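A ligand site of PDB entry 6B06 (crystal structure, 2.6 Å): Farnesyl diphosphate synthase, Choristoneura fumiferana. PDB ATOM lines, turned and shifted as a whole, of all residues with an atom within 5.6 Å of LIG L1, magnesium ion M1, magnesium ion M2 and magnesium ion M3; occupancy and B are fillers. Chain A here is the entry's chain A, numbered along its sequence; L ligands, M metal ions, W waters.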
ATOM      1  N   LEU A  87      -5.976 -17.884   8.049  1.00  0.00           N
ATOM      2  CA  LEU A  87      -5.853 -16.931   6.973  1.00  0.00           C
ATOM      3  C   LEU A  87      -7.208 -16.504   6.496  1.00  0.00           C
ATOM      4  O   LEU A  87      -7.479 -15.315   6.535  1.00  0.00           O
ATOM      5  CB  LEU A  87      -5.038 -17.461   5.821  1.00  0.00           C
ATOM      6  CG  LEU A  87      -3.603 -17.888   6.088  1.00  0.00           C
ATOM      7  CD1 LEU A  87      -3.036 -18.611   4.874  1.00  0.00           C
ATOM      8  CD2 LEU A  87      -2.745 -16.718   6.416  1.00  0.00           C
ATOM      9  N   VAL A  88      -8.102 -17.437   6.139  1.00  0.00           N
ATOM     10  CA  VAL A  88      -9.422 -17.001   5.588  1.00  0.00           C
ATOM     11  C   VAL A  88     -10.317 -16.374   6.632  1.00  0.00           C
ATOM     12  O   VAL A  88     -11.174 -15.625   6.277  1.00  0.00           O
ATOM     13  CB  VAL A  88     -10.272 -18.063   4.831  1.00  0.00           C
ATOM     14  CG1 VAL A  88      -9.418 -18.870   3.860  1.00  0.00           C
ATOM     15  CG2 VAL A  88     -11.066 -18.939   5.753  1.00  0.00           C
ATOM     16  N   ASP A  91      -8.870 -12.904   6.218  1.00  0.00           N
ATOM     17  CA  ASP A  91      -9.200 -12.499   4.832  1.00  0.00           C
ATOM     18  C   ASP A  91     -10.641 -12.054   4.736  1.00  0.00           C
ATOM     19  O   ASP A  91     -10.863 -10.982   4.239  1.00  0.00           O
ATOM     20  CB  ASP A  91      -8.977 -13.601   3.802  1.00  0.00           C
ATOM     21  CG  ASP A  91      -9.125 -13.109   2.365  1.00  0.00           C
ATOM     22  OD1 ASP A  91      -8.130 -12.583   1.808  1.00  0.00           O
ATOM     23  OD2 ASP A  91     -10.217 -13.241   1.757  1.00  0.00           O
ATOM     24  N   ASP A  92     -11.584 -12.842   5.249  1.00  0.00           N
ATOM     25  CA  ASP A  92     -13.000 -12.401   5.296  1.00  0.00           C
ATOM     26  C   ASP A  92     -13.234 -11.054   6.014  1.00  0.00           C
ATOM     27  O   ASP A  92     -14.118 -10.318   5.640  1.00  0.00           O
ATOM     28  CB  ASP A  92     -13.931 -13.474   5.901  1.00  0.00           C
ATOM     29  CG  ASP A  92     -13.858 -14.856   5.159  1.00  0.00           C
ATOM     30  OD1 ASP A  92     -13.667 -14.878   3.910  1.00  0.00           O
ATOM     31  OD2 ASP A  92     -13.964 -15.923   5.850  1.00  0.00           O
ATOM     32  N   ASP A  95     -11.982  -8.266   3.493  1.00  0.00           N
ATOM     33  CA  ASP A  95     -12.695  -8.285   2.240  1.00  0.00           C
ATOM     34  C   ASP A  95     -14.216  -8.078   2.437  1.00  0.00           C
ATOM     35  O   ASP A  95     -14.984  -8.184   1.479  1.00  0.00           O
ATOM     36  CB  ASP A  95     -12.367  -9.635   1.532  1.00  0.00           C
ATOM     37  CG  ASP A  95     -10.885  -9.714   1.070  1.00  0.00           C
ATOM     38  OD1 ASP A  95     -10.138  -8.725   1.256  1.00  0.00           O
ATOM     39  OD2 ASP A  95     -10.443 -10.751   0.524  1.00  0.00           O
ATOM     40  N   SER A  97     -16.440 -10.023   3.569  1.00  0.00           N
ATOM     41  CA  SER A  97     -17.224 -11.179   3.152  1.00  0.00           C
ATOM     42  C   SER A  97     -18.359 -11.407   4.142  1.00  0.00           C
ATOM     43  O   SER A  97     -18.324 -10.899   5.263  1.00  0.00           O
ATOM     44  CB  SER A  97     -16.350 -12.425   3.027  1.00  0.00           C
ATOM     45  OG  SER A  97     -15.520 -12.311   1.859  1.00  0.00           O
ATOM     46  N   ARG A 100     -18.818 -18.187   3.991  1.00  0.00           N
ATOM     47  CA  ARG A 100     -17.747 -19.033   3.520  1.00  0.00           C
ATOM     48  C   ARG A 100     -18.037 -20.506   3.797  1.00  0.00           C
ATOM     49  O   ARG A 100     -18.430 -20.862   4.909  1.00  0.00           O
ATOM     50  CB  ARG A 100     -16.421 -18.654   4.192  1.00  0.00           C
ATOM     51  CG  ARG A 100     -15.351 -19.719   3.917  1.00  0.00           C
ATOM     52  CD  ARG A 100     -13.947 -19.256   4.115  1.00  0.00           C
ATOM     53  NE  ARG A 100     -13.722 -17.947   3.522  1.00  0.00           N
ATOM     54  CZ  ARG A 100     -13.042 -17.691   2.397  1.00  0.00           C
ATOM     55  NH1 ARG A 100     -12.452 -18.652   1.694  1.00  0.00           N
ATOM     56  NH2 ARG A 100     -12.934 -16.420   2.004  1.00  0.00           N
ATOM     57  N   THR A 155       2.603 -15.353   2.955  1.00  0.00           N
ATOM     58  CA  THR A 155       1.178 -15.061   2.889  1.00  0.00           C
ATOM     59  C   THR A 155       0.865 -13.620   3.319  1.00  0.00           C
ATOM     60  O   THR A 155       0.014 -12.964   2.714  1.00  0.00           O
ATOM     61  CB  THR A 155       0.371 -16.110   3.650  1.00  0.00           C
ATOM     62  OG1 THR A 155       0.697 -17.420   3.137  1.00  0.00           O
ATOM     63  CG2 THR A 155      -1.104 -15.891   3.445  1.00  0.00           C
ATOM     64  N   GLN A 159      -0.749 -10.710   0.957  1.00  0.00           N
ATOM     65  CA  GLN A 159      -1.978 -10.064   1.385  1.00  0.00           C
ATOM     66  C   GLN A 159      -1.835  -8.561   1.404  1.00  0.00           C
ATOM     67  O   GLN A 159      -2.779  -7.836   1.162  1.00  0.00           O
ATOM     68  CB  GLN A 159      -2.412 -10.579   2.757  1.00  0.00           C
ATOM     69  CG  GLN A 159      -3.037 -11.972   2.718  1.00  0.00           C
ATOM     70  CD  GLN A 159      -4.418 -11.933   2.106  1.00  0.00           C
ATOM     71  OE1 GLN A 159      -4.566 -11.982   0.889  1.00  0.00           O
ATOM     72  NE2 GLN A 159      -5.424 -11.813   2.933  1.00  0.00           N
ATOM     73  N   ASP A 162      -2.057  -7.210  -2.082  1.00  0.00           N
ATOM     74  CA  ASP A 162      -3.437  -7.304  -2.498  1.00  0.00           C
ATOM     75  C   ASP A 162      -4.279  -6.151  -1.929  1.00  0.00           C
ATOM     76  O   ASP A 162      -5.016  -5.503  -2.670  1.00  0.00           O
ATOM     77  CB  ASP A 162      -3.953  -8.659  -2.013  1.00  0.00           C
ATOM     78  CG  ASP A 162      -5.409  -8.917  -2.344  1.00  0.00           C
ATOM     79  OD1 ASP A 162      -6.294  -8.182  -1.836  1.00  0.00           O
ATOM     80  OD2 ASP A 162      -5.660  -9.934  -3.065  1.00  0.00           O
ATOM     81  N   LYS A 188       0.668 -14.732  -1.866  1.00  0.00           N
ATOM     82  CA  LYS A 188      -0.547 -14.975  -1.053  1.00  0.00           C
ATOM     83  C   LYS A 188      -1.209 -16.346  -1.174  1.00  0.00           C
ATOM     84  O   LYS A 188      -2.013 -16.714  -0.336  1.00  0.00           O
ATOM     85  CB  LYS A 188      -1.617 -13.903  -1.253  1.00  0.00           C
ATOM     86  CG  LYS A 188      -2.514 -14.058  -2.440  1.00  0.00           C
ATOM     87  CD  LYS A 188      -3.787 -13.271  -2.310  1.00  0.00           C
ATOM     88  CE  LYS A 188      -4.423 -13.256  -3.700  1.00  0.00           C
ATOM     89  NZ  LYS A 188      -5.899 -13.191  -3.659  1.00  0.00           N
ATOM     90  N   THR A 189      -0.908 -17.069  -2.235  1.00  0.00           N
ATOM     91  CA  THR A 189      -1.598 -18.337  -2.530  1.00  0.00           C
ATOM     92  C   THR A 189      -0.613 -19.437  -2.827  1.00  0.00           C
ATOM     93  O   THR A 189      -0.631 -20.439  -2.135  1.00  0.00           O
ATOM     94  CB  THR A 189      -2.510 -18.163  -3.733  1.00  0.00           C
ATOM     95  OG1 THR A 189      -3.379 -17.067  -3.451  1.00  0.00           O
ATOM     96  CG2 THR A 189      -3.316 -19.427  -4.014  1.00  0.00           C
ATOM     97  N   TYR A 192       1.788 -21.192   0.299  1.00  0.00           N
ATOM     98  CA  TYR A 192       1.197 -21.967   1.377  1.00  0.00           C
ATOM     99  C   TYR A 192       0.285 -23.057   0.875  1.00  0.00           C
ATOM    100  O   TYR A 192       0.012 -23.986   1.621  1.00  0.00           O
ATOM    101  CB  TYR A 192       0.459 -21.106   2.404  1.00  0.00           C
ATOM    102  CG  TYR A 192      -1.008 -20.909   2.147  1.00  0.00           C
ATOM    103  CD1 TYR A 192      -1.450 -19.854   1.340  1.00  0.00           C
ATOM    104  CD2 TYR A 192      -1.962 -21.715   2.730  1.00  0.00           C
ATOM    105  CE1 TYR A 192      -2.801 -19.660   1.092  1.00  0.00           C
ATOM    106  CE2 TYR A 192      -3.312 -21.520   2.507  1.00  0.00           C
ATOM    107  CZ  TYR A 192      -3.727 -20.480   1.684  1.00  0.00           C
ATOM    108  OH  TYR A 192      -5.051 -20.254   1.439  1.00  0.00           O
ATOM    109  N   GLN A 228      -5.047 -20.044  -8.462  1.00  0.00           N
ATOM    110  CA  GLN A 228      -5.578 -18.742  -8.091  1.00  0.00           C
ATOM    111  C   GLN A 228      -6.289 -18.017  -9.265  1.00  0.00           C
ATOM    112  O   GLN A 228      -7.211 -17.245  -9.036  1.00  0.00           O
ATOM    113  CB  GLN A 228      -4.454 -17.878  -7.479  1.00  0.00           C
ATOM    114  CG  GLN A 228      -4.858 -16.496  -6.987  1.00  0.00           C
ATOM    115  CD  GLN A 228      -5.897 -16.509  -5.884  1.00  0.00           C
ATOM    116  OE1 GLN A 228      -6.952 -15.895  -5.990  1.00  0.00           O
ATOM    117  NE2 GLN A 228      -5.604 -17.230  -4.838  1.00  0.00           N
ATOM    118  N   ASP A 231      -9.624 -19.548  -8.921  1.00  0.00           N
ATOM    119  CA  ASP A 231     -10.325 -18.887  -7.825  1.00  0.00           C
ATOM    120  C   ASP A 231     -10.895 -17.572  -8.292  1.00  0.00           C
ATOM    121  O   ASP A 231     -12.026 -17.244  -7.956  1.00  0.00           O
ATOM    122  CB  ASP A 231      -9.439 -18.620  -6.622  1.00  0.00           C
ATOM    123  CG  ASP A 231     -10.249 -18.047  -5.414  1.00  0.00           C
ATOM    124  OD1 ASP A 231     -11.153 -18.814  -4.980  1.00  0.00           O
ATOM    125  OD2 ASP A 231     -10.005 -16.857  -4.912  1.00  0.00           O
ATOM    126  N   ASP A 232     -10.118 -16.781  -9.031  1.00  0.00           N
ATOM    127  CA  ASP A 232     -10.608 -15.482  -9.536  1.00  0.00           C
ATOM    128  C   ASP A 232     -11.796 -15.619 -10.481  1.00  0.00           C
ATOM    129  O   ASP A 232     -12.817 -14.897 -10.346  1.00  0.00           O
ATOM    130  CB  ASP A 232      -9.480 -14.707 -10.199  1.00  0.00           C
ATOM    131  CG  ASP A 232      -8.477 -14.131  -9.169  1.00  0.00           C
ATOM    132  OD1 ASP A 232      -8.840 -14.088  -7.974  1.00  0.00           O
ATOM    133  OD2 ASP A 232      -7.347 -13.690  -9.537  1.00  0.00           O
ATOM    134  N   ASP A 235     -14.948 -16.449  -8.397  1.00  0.00           N
ATOM    135  CA  ASP A 235     -15.522 -15.325  -7.668  1.00  0.00           C
ATOM    136  C   ASP A 235     -16.579 -14.644  -8.474  1.00  0.00           C
ATOM    137  O   ASP A 235     -17.583 -14.213  -7.936  1.00  0.00           O
ATOM    138  CB  ASP A 235     -14.461 -14.280  -7.347  1.00  0.00           C
ATOM    139  CG  ASP A 235     -14.884 -13.400  -6.223  1.00  0.00           C
ATOM    140  OD1 ASP A 235     -14.799 -13.888  -5.067  1.00  0.00           O
ATOM    141  OD2 ASP A 235     -15.286 -12.245  -6.504  1.00  0.00           O
ATOM    142  N   LYS A 245     -19.507 -19.389  -1.038  1.00  0.00           N
ATOM    143  CA  LYS A 245     -19.129 -17.996  -0.766  1.00  0.00           C
ATOM    144  C   LYS A 245     -19.712 -17.039  -1.817  1.00  0.00           C
ATOM    145  O   LYS A 245     -19.960 -17.422  -2.958  1.00  0.00           O
ATOM    146  CB  LYS A 245     -17.595 -17.844  -0.678  1.00  0.00           C
ATOM    147  CG  LYS A 245     -16.790 -18.556  -1.778  1.00  0.00           C
ATOM    148  CD  LYS A 245     -15.294 -18.160  -1.813  1.00  0.00           C
ATOM    149  CE  LYS A 245     -14.635 -18.501  -3.169  1.00  0.00           C
ATOM    150  NZ  LYS A 245     -13.157 -18.786  -3.121  1.00  0.00           N
ATOM    151  N   THR A 248     -16.833 -11.135  -4.269  1.00  0.00           N
ATOM    152  CA  THR A 248     -16.689  -9.715  -3.854  1.00  0.00           C
ATOM    153  C   THR A 248     -15.507  -8.958  -4.473  1.00  0.00           C
ATOM    154  O   THR A 248     -15.297  -7.789  -4.104  1.00  0.00           O
ATOM    155  CB  THR A 248     -16.640  -9.519  -2.281  1.00  0.00           C
ATOM    156  OG1 THR A 248     -15.298  -9.687  -1.753  1.00  0.00           O
ATOM    157  CG2 THR A 248     -17.602 -10.459  -1.554  1.00  0.00           C
ATOM    158  N   ASP A 249     -14.758  -9.575  -5.383  1.00  0.00           N
ATOM    159  CA  ASP A 249     -13.596  -8.918  -5.994  1.00  0.00           C
ATOM    160  C   ASP A 249     -14.005  -7.639  -6.740  1.00  0.00           C
ATOM    161  O   ASP A 249     -13.239  -6.657  -6.751  1.00  0.00           O
ATOM    162  CB  ASP A 249     -12.833  -9.849  -6.954  1.00  0.00           C
ATOM    163  CG  ASP A 249     -12.340 -11.179  -6.293  1.00  0.00           C
ATOM    164  OD1 ASP A 249     -12.540 -11.398  -5.088  1.00  0.00           O
ATOM    165  OD2 ASP A 249     -11.775 -12.032  -7.023  1.00  0.00           O
ATOM    166  N   LYS A 254     -10.718  -5.448  -6.422  1.00  0.00           N
ATOM    167  CA  LYS A 254      -9.481  -6.215  -6.335  1.00  0.00           C
ATOM    168  C   LYS A 254      -8.884  -6.332  -7.715  1.00  0.00           C
ATOM    169  O   LYS A 254      -9.611  -6.320  -8.723  1.00  0.00           O
ATOM    170  CB  LYS A 254      -9.696  -7.609  -5.773  1.00  0.00           C
ATOM    171  CG  LYS A 254     -10.186  -7.670  -4.351  1.00  0.00           C
ATOM    172  CD  LYS A 254      -9.109  -7.264  -3.353  1.00  0.00           C
ATOM    173  CE  LYS A 254      -9.484  -7.766  -1.958  1.00  0.00           C
ATOM    174  NZ  LYS A 254      -9.028  -6.837  -0.882  1.00  0.00           N
HETATM  175  O1  LIG L   1      -9.361 -14.078  -3.282  1.00  0.00           O
HETATM  176  P1  LIG L   1      -8.931 -14.276  -1.820  1.00  0.00           P
HETATM  177  O2  LIG L   1      -9.962 -13.368  -0.862  1.00  0.00           O
HETATM  178  O3  LIG L   1      -7.558 -13.917  -1.741  1.00  0.00           O
HETATM  179  C1  LIG L   1      -9.324 -15.951  -1.260  1.00  0.00           C
HETATM  180  P2  LIG L   1     -11.143 -16.075  -1.266  1.00  0.00           P
HETATM  181  O4  LIG L   1     -11.448 -17.544  -0.626  1.00  0.00           O
HETATM  182  O5  LIG L   1     -11.639 -14.952  -0.212  1.00  0.00           O
HETATM  183  O6  LIG L   1     -11.736 -15.902  -2.618  1.00  0.00           O
HETATM  184  C2  LIG L   1      -8.869 -16.091   0.167  1.00  0.00           C
HETATM  185  C3  LIG L   1      -7.450 -16.117   0.374  1.00  0.00           C
HETATM  186  C4  LIG L   1      -7.121 -15.847   1.689  1.00  0.00           C
HETATM  187  C5  LIG L   1      -5.833 -15.820   2.163  1.00  0.00           C
HETATM  188  C6  LIG L   1      -4.798 -16.073   1.319  1.00  0.00           C
HETATM  189  C7  LIG L   1      -5.091 -16.349   0.019  1.00  0.00           C
HETATM  190  N1  LIG L   1      -6.388 -16.392  -0.441  1.00  0.00           N
HETATM  191  C8  LIG L   1      -6.344 -16.665  -1.903  1.00  0.00           C
HETATM  192  C1  LG2 L   2      -9.732 -20.646  -0.379  1.00  0.00           C
HETATM  193  O1  LG2 L   2      -9.134 -21.855  -0.868  1.00  0.00           O
HETATM  194  C2  LG2 L   2      -8.714 -19.540  -0.341  1.00  0.00           C
HETATM  195  C3  LG2 L   2      -7.934 -19.500  -1.624  1.00  0.00           C
HETATM  196  C4  LG2 L   2      -6.605 -19.531  -1.619  1.00  0.00           C
HETATM  197  C5  LG2 L   2      -8.699 -19.424  -2.900  1.00  0.00           C
HETATM  198  P1  LG2 L   2     -10.093 -23.120  -1.179  1.00  0.00           P
HETATM  199  O2  LG2 L   2     -11.023 -22.596  -2.260  1.00  0.00           O
HETATM  200  O3  LG2 L   2      -9.280 -24.409  -1.306  1.00  0.00           O
HETATM  201  O4  LG2 L   2     -10.986 -23.245   0.179  1.00  0.00           O
HETATM  202  P2  LG2 L   2     -11.524 -24.576   0.949  1.00  0.00           P
HETATM  203  O5  LG2 L   2     -11.727 -25.651  -0.106  1.00  0.00           O
HETATM  204  O6  LG2 L   2     -12.843 -24.023   1.473  1.00  0.00           O
HETATM  205  O7  LG2 L   2     -10.450 -24.960   1.981  1.00  0.00           O
HETATM  206 MG    MG M   1      -8.568 -11.489  -0.354  1.00  0.00          MG
HETATM  207 MG    MG M   2     -11.831 -12.818  -0.320  1.00  0.00          MG
HETATM  208 MG    MG M   3     -11.492 -14.609  -4.293  1.00  0.00          MG
HETATM  209  O   HOH W   1     -12.970 -12.829   1.389  1.00  0.00           O
HETATM  210  O   HOH W   2     -10.833 -14.159  -5.899  1.00  0.00           O
HETATM  211  O   HOH W   3      -7.749 -10.043   0.974  1.00  0.00           O
HETATM  212  O   HOH W   4     -12.630 -10.273  -2.239  1.00  0.00           O
HETATM  213  O   HOH W   5     -12.863 -16.277  -5.002  1.00  0.00           O
HETATM  214  O   HOH W   6     -14.177 -15.078  -0.846  1.00  0.00           O
HETATM  215  O   HOH W   7     -12.514 -13.154  -2.845  1.00  0.00           O
HETATM  216  O   HOH W   8      -6.556 -12.265  -0.677  1.00  0.00           O
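The side-chain amino group of Lys 188 lies within salt-bridge range of an oxygen (O3) of LIG L1 (2.6 Å). The guanidinium group (NH1) of Arg 100 is in salt-bridge range of an oxygen (O4) of LIG L1, at 2.8 Å. O4 of LIG L1 lies within salt-bridge range of NZ of Lys 245, at 3.3 Å.
NZ of Lys 254 is in salt-bridge range of OD1 of Asp 95 (3.1 Å). The side-chain carboxylate (OD1) of Asp 91 sits close to the side-chain amide nitrogen (NE2) of Gln 159 (3.0 Å). NZ of Lys 188 lies within salt-bridge range of OD2 of Asp 162. The side-chain carboxylate (OD1) of Asp 92 is in salt-bridge range of the guanidinium group (NH2) of Arg 100, at 2.6 Å. The side-chain carboxylate (OD1) of Asp 231 is in salt-bridge range of the side-chain amino group (NZ) of Lys 245 (2.7 Å). The side-chain hydroxyl (OG1) of Thr 189 sits at hydrogen-bond distance from the side-chain amide nitrogen (NE2) of Gln 228 (2.6 Å). OE1 of Gln 228 sits close to OD1 of Asp 232 (3.3 Å). OD2 of Asp 235 lies within hydrogen-bond range of N of Asp 249 (2.9 Å).
Merely in contact with LIG L1: Thr 189 (3.4 Å) and Gln 228 (3.1 Å). The nearest printed residue that does not touch LIG L1 is Leu 87 (4.1 Å).
Within 4 Å of magnesium ion M1: Asp 91 and Asp 95. The nearest printed residue that does not touch magnesium ion M1 is Lys 254 (4.2 Å).
Two residues have an atom within 4 Å of magnesium ion M2: Asp 91 and Asp 95. The nearest printed residue that does not touch magnesium ion M2 is Ser 97 (4.3 Å).
Merely in contact with magnesium ion M3: Asp 249 and Asp 235. Of the 21 residues printed, 3 come within 4 Å of magnesium ion M3.
Magnesium ion M1 is bound by water W3 (2.1 Å), water W8 (2.2 Å), the side-chain carboxylate of Asp 95 (2.2 Å), an oxygen (O2) of LIG L1 (2.4 Å) and the side-chain carboxylate of Asp 91 (2.5 Å).
Magnesium ion M2 is bound by an oxygen (O2) of LIG L1 (2.0 Å), water W1 (2.1 Å) and an oxygen (O5) of LIG L1 (2.1 Å). Magnesium ion M2 has three donor atoms within binding distance. Slightly farther from magnesium ion M2 lies OD2 of Asp 95 (2.6 Å). Slightly farther from magnesium ion M2 lies water W7 (2.6 Å). Slightly farther from magnesium ion M2 lies the side-chain carboxylate (OD2) of Asp 91 (2.7 Å).
Magnesium ion M3 is bound by water W2 (1.8 Å), O6 of LIG L1 (2.1 Å), water W5 (2.3 Å), water W7 (2.3 Å) and O1 of LIG L1 (2.4 Å). Magnesium ion M3 has five donor atoms within binding distance. Slightly farther from magnesium ion M3 lies OD2 of Asp 231 (2.8 Å).
Water W8 lies within hydrogen-bond range of the side-chain amide oxygen of Gln 159 (2.5 Å), the side-chain amino group of Lys 188 (3.2 Å) and the side-chain carboxylate of Asp 162 (3.5 Å). Water W1 lies within hydrogen-bond range of the side-chain hydroxyl of Ser 97 (2.6 Å), the side-chain carboxylate of Asp 91 (2.8 Å) and the side-chain carboxylate of Asp 92 (3.3 Å). Water W7 bridges the side-chain carboxylate (OD1) of Asp 249 and the side-chain carboxylate (OD1) of Asp 235. Water W5 lies within hydrogen-bond range of the side-chain carboxylate of Asp 231 (2.9 Å), the side-chain carboxylate of Asp 235 (3.1 Å) and the side-chain amino group of Lys 245 (3.1 Å). Water W4 bridges OG1 of Thr 248 and OD1 of Asp 249.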
